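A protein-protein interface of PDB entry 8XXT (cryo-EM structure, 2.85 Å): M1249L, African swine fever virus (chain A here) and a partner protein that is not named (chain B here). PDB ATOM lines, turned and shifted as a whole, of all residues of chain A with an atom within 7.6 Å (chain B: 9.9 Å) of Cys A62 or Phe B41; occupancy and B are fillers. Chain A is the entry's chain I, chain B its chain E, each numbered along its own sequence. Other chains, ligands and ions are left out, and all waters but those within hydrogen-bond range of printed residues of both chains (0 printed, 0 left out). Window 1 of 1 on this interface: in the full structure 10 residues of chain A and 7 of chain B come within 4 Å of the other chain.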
ATOM      1  N   PHE A  58      18.149   8.523  17.532  1.00  0.00           N
ATOM      2  CA  PHE A  58      16.964   8.363  18.359  1.00  0.00           C
ATOM      3  C   PHE A  58      16.907   6.960  18.945  1.00  0.00           C
ATOM      4  O   PHE A  58      17.496   6.017  18.412  1.00  0.00           O
ATOM      5  CB  PHE A  58      15.695   8.637  17.551  1.00  0.00           C
ATOM      6  CG  PHE A  58      15.335  10.092  17.458  1.00  0.00           C
ATOM      7  CD1 PHE A  58      16.139  11.058  18.035  1.00  0.00           C
ATOM      8  CD2 PHE A  58      14.192  10.491  16.789  1.00  0.00           C
ATOM      9  CE1 PHE A  58      15.807  12.396  17.949  1.00  0.00           C
ATOM     10  CE2 PHE A  58      13.854  11.827  16.698  1.00  0.00           C
ATOM     11  CZ  PHE A  58      14.661  12.780  17.279  1.00  0.00           C
ATOM     12  N   SER A  59      16.194   6.833  20.060  1.00  0.00           N
ATOM     13  CA  SER A  59      15.971   5.500  20.601  1.00  0.00           C
ATOM     14  C   SER A  59      14.672   4.924  20.048  1.00  0.00           C
ATOM     15  O   SER A  59      13.702   5.662  19.853  1.00  0.00           O
ATOM     16  CB  SER A  59      15.904   5.537  22.123  1.00  0.00           C
ATOM     17  OG  SER A  59      14.701   6.143  22.562  1.00  0.00           O
ATOM     18  N   PRO A  60      14.629   3.617  19.780  1.00  0.00           N
ATOM     19  CA  PRO A  60      13.383   3.020  19.274  1.00  0.00           C
ATOM     20  C   PRO A  60      12.221   3.153  20.241  1.00  0.00           C
ATOM     21  O   PRO A  60      11.058   3.140  19.811  1.00  0.00           O
ATOM     22  CB  PRO A  60      13.766   1.551  19.044  1.00  0.00           C
ATOM     23  CG  PRO A  60      14.956   1.322  19.920  1.00  0.00           C
ATOM     24  CD  PRO A  60      15.698   2.621  19.951  1.00  0.00           C
ATOM     25  N   GLN A  61      12.503   3.285  21.539  1.00  0.00           N
ATOM     26  CA  GLN A  61      11.437   3.478  22.513  1.00  0.00           C
ATOM     27  C   GLN A  61      10.688   4.780  22.273  1.00  0.00           C
ATOM     28  O   GLN A  61       9.502   4.882  22.595  1.00  0.00           O
ATOM     29  CB  GLN A  61      12.012   3.444  23.929  1.00  0.00           C
ATOM     30  CG  GLN A  61      13.110   2.409  24.137  1.00  0.00           C
ATOM     31  CD  GLN A  61      12.621   0.975  24.015  1.00  0.00           C
ATOM     32  OE1 GLN A  61      11.419   0.712  23.977  1.00  0.00           O
ATOM     33  NE2 GLN A  61      13.559   0.037  23.956  1.00  0.00           N
ATOM     34  N   CYS A  62      11.353   5.779  21.690  1.00  0.00           N
ATOM     35  CA  CYS A  62      10.688   7.041  21.381  1.00  0.00           C
ATOM     36  C   CYS A  62       9.644   6.862  20.283  1.00  0.00           C
ATOM     37  O   CYS A  62       8.505   7.346  20.396  1.00  0.00           O
ATOM     38  CB  CYS A  62      11.735   8.078  20.979  1.00  0.00           C
ATOM     39  SG  CYS A  62      11.072   9.628  20.388  1.00  0.00           S
ATOM     40  N   PHE A  63      10.014   6.167  19.204  1.00  0.00           N
ATOM     41  CA  PHE A  63       9.033   5.864  18.173  1.00  0.00           C
ATOM     42  C   PHE A  63       7.933   4.972  18.723  1.00  0.00           C
ATOM     43  O   PHE A  63       6.770   5.107  18.330  1.00  0.00           O
ATOM     44  CB  PHE A  63       9.691   5.196  16.968  1.00  0.00           C
ATOM     45  CG  PHE A  63       8.716   4.824  15.889  1.00  0.00           C
ATOM     46  CD1 PHE A  63       8.160   5.800  15.080  1.00  0.00           C
ATOM     47  CD2 PHE A  63       8.316   3.513  15.713  1.00  0.00           C
ATOM     48  CE1 PHE A  63       7.255   5.469  14.095  1.00  0.00           C
ATOM     49  CE2 PHE A  63       7.408   3.177  14.729  1.00  0.00           C
ATOM     50  CZ  PHE A  63       6.876   4.157  13.921  1.00  0.00           C
ATOM     51  N   MET A  64       8.282   4.057  19.632  1.00  0.00           N
ATOM     52  CA  MET A  64       7.262   3.260  20.304  1.00  0.00           C
ATOM     53  C   MET A  64       6.279   4.146  21.053  1.00  0.00           C
ATOM     54  O   MET A  64       5.066   3.922  21.000  1.00  0.00           O
ATOM     55  CB  MET A  64       7.920   2.267  21.258  1.00  0.00           C
ATOM     56  CG  MET A  64       8.077   0.903  20.652  1.00  0.00           C
ATOM     57  SD  MET A  64       6.593   0.468  19.738  1.00  0.00           S
ATOM     58  CE  MET A  64       7.291   0.172  18.126  1.00  0.00           C
ATOM     59  N   ARG A  65       6.788   5.159  21.752  1.00  0.00           N
ATOM     60  CA  ARG A  65       5.922   6.080  22.476  1.00  0.00           C
ATOM     61  C   ARG A  65       4.955   6.777  21.531  1.00  0.00           C
ATOM     62  O   ARG A  65       3.741   6.802  21.771  1.00  0.00           O
ATOM     63  CB  ARG A  65       6.767   7.107  23.228  1.00  0.00           C
ATOM     64  CG  ARG A  65       7.130   6.690  24.635  1.00  0.00           C
ATOM     65  CD  ARG A  65       5.910   6.738  25.546  1.00  0.00           C
ATOM     66  NE  ARG A  65       5.698   8.032  26.192  1.00  0.00           N
ATOM     67  CZ  ARG A  65       6.589   8.685  26.928  1.00  0.00           C
ATOM     68  NH1 ARG A  65       7.776   8.172  27.206  1.00  0.00           N
ATOM     69  NH2 ARG A  65       6.271   9.880  27.418  1.00  0.00           N
ATOM     70  N   MET A  66       5.471   7.344  20.438  1.00  0.00           N
ATOM     71  CA  MET A  66       4.575   8.105  19.568  1.00  0.00           C
ATOM     72  C   MET A  66       3.607   7.202  18.817  1.00  0.00           C
ATOM     73  O   MET A  66       2.485   7.622  18.511  1.00  0.00           O
ATOM     74  CB  MET A  66       5.348   8.960  18.575  1.00  0.00           C
ATOM     75  CG  MET A  66       6.605   8.356  18.070  1.00  0.00           C
ATOM     76  SD  MET A  66       7.681   9.678  17.537  1.00  0.00           S
ATOM     77  CE  MET A  66       6.526  10.685  16.614  1.00  0.00           C
ATOM     78  N   ALA A  67       4.015   5.974  18.495  1.00  0.00           N
ATOM     79  CA  ALA A  67       3.086   5.041  17.871  1.00  0.00           C
ATOM     80  C   ALA A  67       2.024   4.579  18.857  1.00  0.00           C
ATOM     81  O   ALA A  67       0.882   4.319  18.463  1.00  0.00           O
ATOM     82  CB  ALA A  67       3.850   3.849  17.300  1.00  0.00           C
ATOM     83  N   GLU A  68       2.385   4.467  20.138  1.00  0.00           N
ATOM     84  CA  GLU A  68       1.402   4.188  21.177  1.00  0.00           C
ATOM     85  C   GLU A  68       0.398   5.325  21.292  1.00  0.00           C
ATOM     86  O   GLU A  68      -0.805   5.090  21.452  1.00  0.00           O
ATOM     87  CB  GLU A  68       2.118   3.956  22.506  1.00  0.00           C
ATOM     88  CG  GLU A  68       1.210   3.617  23.669  1.00  0.00           C
ATOM     89  CD  GLU A  68       1.988   3.349  24.940  1.00  0.00           C
ATOM     90  OE1 GLU A  68       2.461   2.208  25.122  1.00  0.00           O
ATOM     91  OE2 GLU A  68       2.136   4.283  25.754  1.00  0.00           O
ATOM     92  N   ILE A  69       0.878   6.569  21.216  1.00  0.00           N
ATOM     93  CA  ILE A  69      -0.029   7.711  21.146  1.00  0.00           C
ATOM     94  C   ILE A  69      -0.895   7.613  19.898  1.00  0.00           C
ATOM     95  O   ILE A  69      -2.109   7.839  19.945  1.00  0.00           O
ATOM     96  CB  ILE A  69       0.765   9.027  21.185  1.00  0.00           C
ATOM     97  CG1 ILE A  69       1.623   9.087  22.447  1.00  0.00           C
ATOM     98  CG2 ILE A  69      -0.168  10.217  21.117  1.00  0.00           C
ATOM     99  CD1 ILE A  69       2.766  10.060  22.359  1.00  0.00           C
ATOM    100  N   PHE A  72       0.325  11.030  15.632  1.00  0.00           N
ATOM    101  CA  PHE A  72       1.287  11.866  14.935  1.00  0.00           C
ATOM    102  C   PHE A  72       1.115  11.738  13.426  1.00  0.00           C
ATOM    103  O   PHE A  72       0.711  10.693  12.909  1.00  0.00           O
ATOM    104  CB  PHE A  72       2.708  11.486  15.338  1.00  0.00           C
ATOM    105  CG  PHE A  72       3.098  11.967  16.702  1.00  0.00           C
ATOM    106  CD1 PHE A  72       2.783  11.228  17.827  1.00  0.00           C
ATOM    107  CD2 PHE A  72       3.784  13.158  16.861  1.00  0.00           C
ATOM    108  CE1 PHE A  72       3.141  11.668  19.083  1.00  0.00           C
ATOM    109  CE2 PHE A  72       4.146  13.602  18.116  1.00  0.00           C
ATOM    110  CZ  PHE A  72       3.824  12.855  19.227  1.00  0.00           C
ATOM    111  N   LEU A  77       6.281  11.111  12.100  1.00  0.00           N
ATOM    112  CA  LEU A  77       6.549   9.706  12.379  1.00  0.00           C
ATOM    113  C   LEU A  77       7.727   9.202  11.558  1.00  0.00           C
ATOM    114  O   LEU A  77       8.611   8.515  12.082  1.00  0.00           O
ATOM    115  CB  LEU A  77       5.308   8.860  12.094  1.00  0.00           C
ATOM    116  CG  LEU A  77       4.286   8.731  13.219  1.00  0.00           C
ATOM    117  CD1 LEU A  77       3.014   8.086  12.698  1.00  0.00           C
ATOM    118  CD2 LEU A  77       4.857   7.941  14.380  1.00  0.00           C
ATOM    119  N   VAL A  80      10.992  10.630  12.960  1.00  0.00           N
ATOM    120  CA  VAL A  80      11.487   9.965  14.162  1.00  0.00           C
ATOM    121  C   VAL A  80      11.988   8.564  13.840  1.00  0.00           C
ATOM    122  O   VAL A  80      13.007   8.116  14.383  1.00  0.00           O
ATOM    123  CB  VAL A  80      10.404   9.945  15.250  1.00  0.00           C
ATOM    124  CG1 VAL A  80      10.932   9.247  16.493  1.00  0.00           C
ATOM    125  CG2 VAL A  80       9.982  11.359  15.573  1.00  0.00           C
ATOM    126  N   ALA A  81      11.289   7.846  12.958  1.00  0.00           N
ATOM    127  CA  ALA A  81      11.747   6.519  12.567  1.00  0.00           C
ATOM    128  C   ALA A  81      13.110   6.582  11.892  1.00  0.00           C
ATOM    129  O   ALA A  81      13.969   5.731  12.150  1.00  0.00           O
ATOM    130  CB  ALA A  81      10.721   5.861  11.646  1.00  0.00           C
ATOM    131  N   ALA A  84      16.009   7.028  14.398  1.00  0.00           N
ATOM    132  CA  ALA A  84      16.524   5.740  14.821  1.00  0.00           C
ATOM    133  C   ALA A  84      16.872   4.903  13.590  1.00  0.00           C
ATOM    134  O   ALA A  84      16.845   5.380  12.453  1.00  0.00           O
ATOM    135  CB  ALA A  84      15.512   5.037  15.721  1.00  0.00           C
ATOM    136  N   LYS A 151       5.045  -5.955  19.651  1.00  0.00           N
ATOM    137  CA  LYS A 151       5.395  -5.701  21.045  1.00  0.00           C
ATOM    138  C   LYS A 151       4.273  -6.124  21.980  1.00  0.00           C
ATOM    139  O   LYS A 151       4.527  -6.732  23.026  1.00  0.00           O
ATOM    140  CB  LYS A 151       5.741  -4.230  21.260  1.00  0.00           C
ATOM    141  CG  LYS A 151       6.792  -4.020  22.339  1.00  0.00           C
ATOM    142  CD  LYS A 151       7.447  -2.659  22.234  1.00  0.00           C
ATOM    143  CE  LYS A 151       8.795  -2.769  21.543  1.00  0.00           C
ATOM    144  NZ  LYS A 151       9.671  -1.602  21.826  1.00  0.00           N
ATOM    145  N   PRO B  35      15.122  19.241  19.987  1.00  0.00           N
ATOM    146  CA  PRO B  35      14.199  18.354  19.272  1.00  0.00           C
ATOM    147  C   PRO B  35      12.810  18.435  19.878  1.00  0.00           C
ATOM    148  O   PRO B  35      12.649  18.939  20.995  1.00  0.00           O
ATOM    149  CB  PRO B  35      14.826  16.972  19.467  1.00  0.00           C
ATOM    150  CG  PRO B  35      15.457  17.065  20.816  1.00  0.00           C
ATOM    151  CD  PRO B  35      15.873  18.511  21.023  1.00  0.00           C
ATOM    152  N   SER B  36      11.801  17.946  19.166  1.00  0.00           N
ATOM    153  CA  SER B  36      10.434  17.969  19.662  1.00  0.00           C
ATOM    154  C   SER B  36       9.949  16.606  20.124  1.00  0.00           C
ATOM    155  O   SER B  36       8.809  16.494  20.587  1.00  0.00           O
ATOM    156  CB  SER B  36       9.486  18.511  18.584  1.00  0.00           C
ATOM    157  OG  SER B  36       8.242  18.888  19.145  1.00  0.00           O
ATOM    158  N   ILE B  37      10.769  15.564  20.001  1.00  0.00           N
ATOM    159  CA  ILE B  37      10.315  14.213  20.306  1.00  0.00           C
ATOM    160  C   ILE B  37      11.166  13.590  21.405  1.00  0.00           C
ATOM    161  O   ILE B  37      10.680  12.762  22.184  1.00  0.00           O
ATOM    162  CB  ILE B  37      10.326  13.334  19.045  1.00  0.00           C
ATOM    163  CG1 ILE B  37      10.009  14.160  17.795  1.00  0.00           C
ATOM    164  CG2 ILE B  37       9.298  12.249  19.178  1.00  0.00           C
ATOM    165  CD1 ILE B  37       8.602  14.744  17.770  1.00  0.00           C
ATOM    166  N   CYS B  38      12.441  13.976  21.481  1.00  0.00           N
ATOM    167  CA  CYS B  38      13.293  13.466  22.550  1.00  0.00           C
ATOM    168  C   CYS B  38      12.883  14.042  23.899  1.00  0.00           C
ATOM    169  O   CYS B  38      12.825  13.317  24.898  1.00  0.00           O
ATOM    170  CB  CYS B  38      14.760  13.783  22.254  1.00  0.00           C
ATOM    171  SG  CYS B  38      15.732  14.272  23.702  1.00  0.00           S
ATOM    172  N   GLU B  39      12.601  15.339  23.943  1.00  0.00           N
ATOM    173  CA  GLU B  39      12.040  15.978  25.120  1.00  0.00           C
ATOM    174  C   GLU B  39      10.521  16.056  24.963  1.00  0.00           C
ATOM    175  O   GLU B  39       9.937  15.458  24.055  1.00  0.00           O
ATOM    176  CB  GLU B  39      12.677  17.350  25.332  1.00  0.00           C
ATOM    177  CG  GLU B  39      12.401  18.346  24.220  1.00  0.00           C
ATOM    178  CD  GLU B  39      12.207  19.759  24.737  1.00  0.00           C
ATOM    179  OE1 GLU B  39      12.083  19.933  25.967  1.00  0.00           O
ATOM    180  OE2 GLU B  39      12.186  20.698  23.913  1.00  0.00           O
ATOM    181  N   GLY B  40       9.865  16.800  25.847  1.00  0.00           N
ATOM    182  CA  GLY B  40       8.422  16.898  25.799  1.00  0.00           C
ATOM    183  C   GLY B  40       7.741  15.599  26.175  1.00  0.00           C
ATOM    184  O   GLY B  40       8.063  15.003  27.208  1.00  0.00           O
ATOM    185  N   PHE B  41       6.804  15.151  25.341  1.00  0.00           N
ATOM    186  CA  PHE B  41       6.007  13.955  25.606  1.00  0.00           C
ATOM    187  C   PHE B  41       5.330  14.043  26.974  1.00  0.00           C
ATOM    188  O   PHE B  41       5.624  13.293  27.905  1.00  0.00           O
ATOM    189  CB  PHE B  41       6.853  12.684  25.492  1.00  0.00           C
ATOM    190  CG  PHE B  41       6.912  12.124  24.105  1.00  0.00           C
ATOM    191  CD1 PHE B  41       5.803  12.179  23.279  1.00  0.00           C
ATOM    192  CD2 PHE B  41       8.064  11.528  23.630  1.00  0.00           C
ATOM    193  CE1 PHE B  41       5.848  11.665  22.002  1.00  0.00           C
ATOM    194  CE2 PHE B  41       8.113  11.008  22.354  1.00  0.00           C
ATOM    195  CZ  PHE B  41       7.003  11.076  21.540  1.00  0.00           C
ATOM    196  N   VAL B  42       4.415  15.010  27.071  1.00  0.00           N
ATOM    197  CA  VAL B  42       3.605  15.139  28.276  1.00  0.00           C
ATOM    198  C   VAL B  42       2.770  13.884  28.485  1.00  0.00           C
ATOM    199  O   VAL B  42       2.494  13.493  29.625  1.00  0.00           O
ATOM    200  CB  VAL B  42       2.728  16.402  28.193  1.00  0.00           C
ATOM    201  CG1 VAL B  42       2.069  16.685  29.531  1.00  0.00           C
ATOM    202  CG2 VAL B  42       3.560  17.588  27.745  1.00  0.00           C
ATOM    203  N   GLN B  43       2.362  13.235  27.397  1.00  0.00           N
ATOM    204  CA  GLN B  43       1.676  11.955  27.487  1.00  0.00           C
ATOM    205  C   GLN B  43       2.543  10.926  28.195  1.00  0.00           C
ATOM    206  O   GLN B  43       3.724  10.764  27.877  1.00  0.00           O
ATOM    207  CB  GLN B  43       1.315  11.461  26.087  1.00  0.00           C
ATOM    208  CG  GLN B  43       0.538  10.161  26.050  1.00  0.00           C
ATOM    209  CD  GLN B  43      -0.910  10.345  25.664  1.00  0.00           C
ATOM    210  OE1 GLN B  43      -1.817  10.003  26.420  1.00  0.00           O
ATOM    211  NE2 GLN B  43      -1.136  10.924  24.498  1.00  0.00           N
ATOM    212  N   ALA B  44       1.954  10.229  29.161  1.00  0.00           N
ATOM    213  CA  ALA B  44       2.649   9.155  29.850  1.00  0.00           C
ATOM    214  C   ALA B  44       2.452   7.840  29.109  1.00  0.00           C
ATOM    215  O   ALA B  44       1.389   7.576  28.540  1.00  0.00           O
ATOM    216  CB  ALA B  44       2.154   9.027  31.289  1.00  0.00           C
ATOM    217  N   SER B  45       3.496   7.016  29.113  1.00  0.00           N
ATOM    218  CA  SER B  45       3.427   5.731  28.434  1.00  0.00           C
ATOM    219  C   SER B  45       2.354   4.858  29.065  1.00  0.00           C
ATOM    220  O   SER B  45       2.222   4.798  30.290  1.00  0.00           O
ATOM    221  CB  SER B  45       4.781   5.027  28.498  1.00  0.00           C
ATOM    222  OG  SER B  45       5.061   4.576  29.811  1.00  0.00           O
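The side-chain hydroxyl (OG) of Ser A59 is in hydrogen-bond range of the backbone NH (N) of Cys A62.
SG of Cys A62 lies close to O of Ile B37 (3.6 Å).
The backbone carbonyl oxygen (O) of Gln B43 is in hydrogen-bond range of the guanidinium group (NH2) of Arg A65, at 2.7 Å.
No residue of chain B comes within 4 Å of Ser A59.
Cys A62 touches just these residues of chain B: Ile B37 and Phe B41.
Of chain B, only Phe B41, Gln B43 and Ser B45 come within 4 Å of Arg A65.
Ala A84 touches none of the printed residues of chain B.
Of the printed residues of chain A, Ile B37 touches Cys A62, Met A66 and Val A80.
Glu B39 touches none of the printed residues of chain A.
No residue of chain A comes within 4 Å of Gly B40.
Printed residues of chain A within 4 Å of Phe B41: Cys A62 (3.8 Å), Arg A65 (3.5 Å), Ile A69 (3.5 Å) and Phe A72 (3.6 Å).
Printed residues of chain A within 4 Å of Gln B43: Arg A65 and Ile A69.
Printed residues of chain A within 4 Å of Ser B45: Arg A65 (3.6 Å) and Glu A68 (3.3 Å).
The nearest residue of chain B that does not touch Cys A62 is Cys B38 (4.7 Å).
The nearest printed residue of chain A that does not touch Phe B41 is Met A66 (4.001 Å).
Cys A62 touches Phe B41.
NH2 of Arg A65 touches CB of Phe B41 (3.5 Å).
Arg A65 touches Ser B45.
CG2 of Ile B37 touches SD of Met A66, 3.5 Å away.
Ser B45 touches Glu A68 (CA to OE2, 3.3 Å).
Phe B41 touches Ile A69 (CE1 to CD1, 3.5 Å).
CG2 of Ile A69 touches NE2 of Gln B43, 3.6 Å away.
Phe A72 touches Phe B41.
CG2 of Val A80 touches CG1 of Ile B37, at 3.6 Å.
Hydrophobic or aromatic side chains of chain A within 4 Å of the printed part of chain B: Met A66, Ile A69, Phe A72 and Val A80.
Of the 11 printed residues of chain B, 4 touch a printed residue of chain A.
Hydrophobic or aromatic side chains of chain B that line the printed part of chain A: Ile B37 and Phe B41.
Among the printed residues, 11 pairs touch across the chains.
Among the printed residues, no Asp or Glu carboxylate lies within 4 Å of a Lys or Arg side-chain nitrogen of the other chain.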
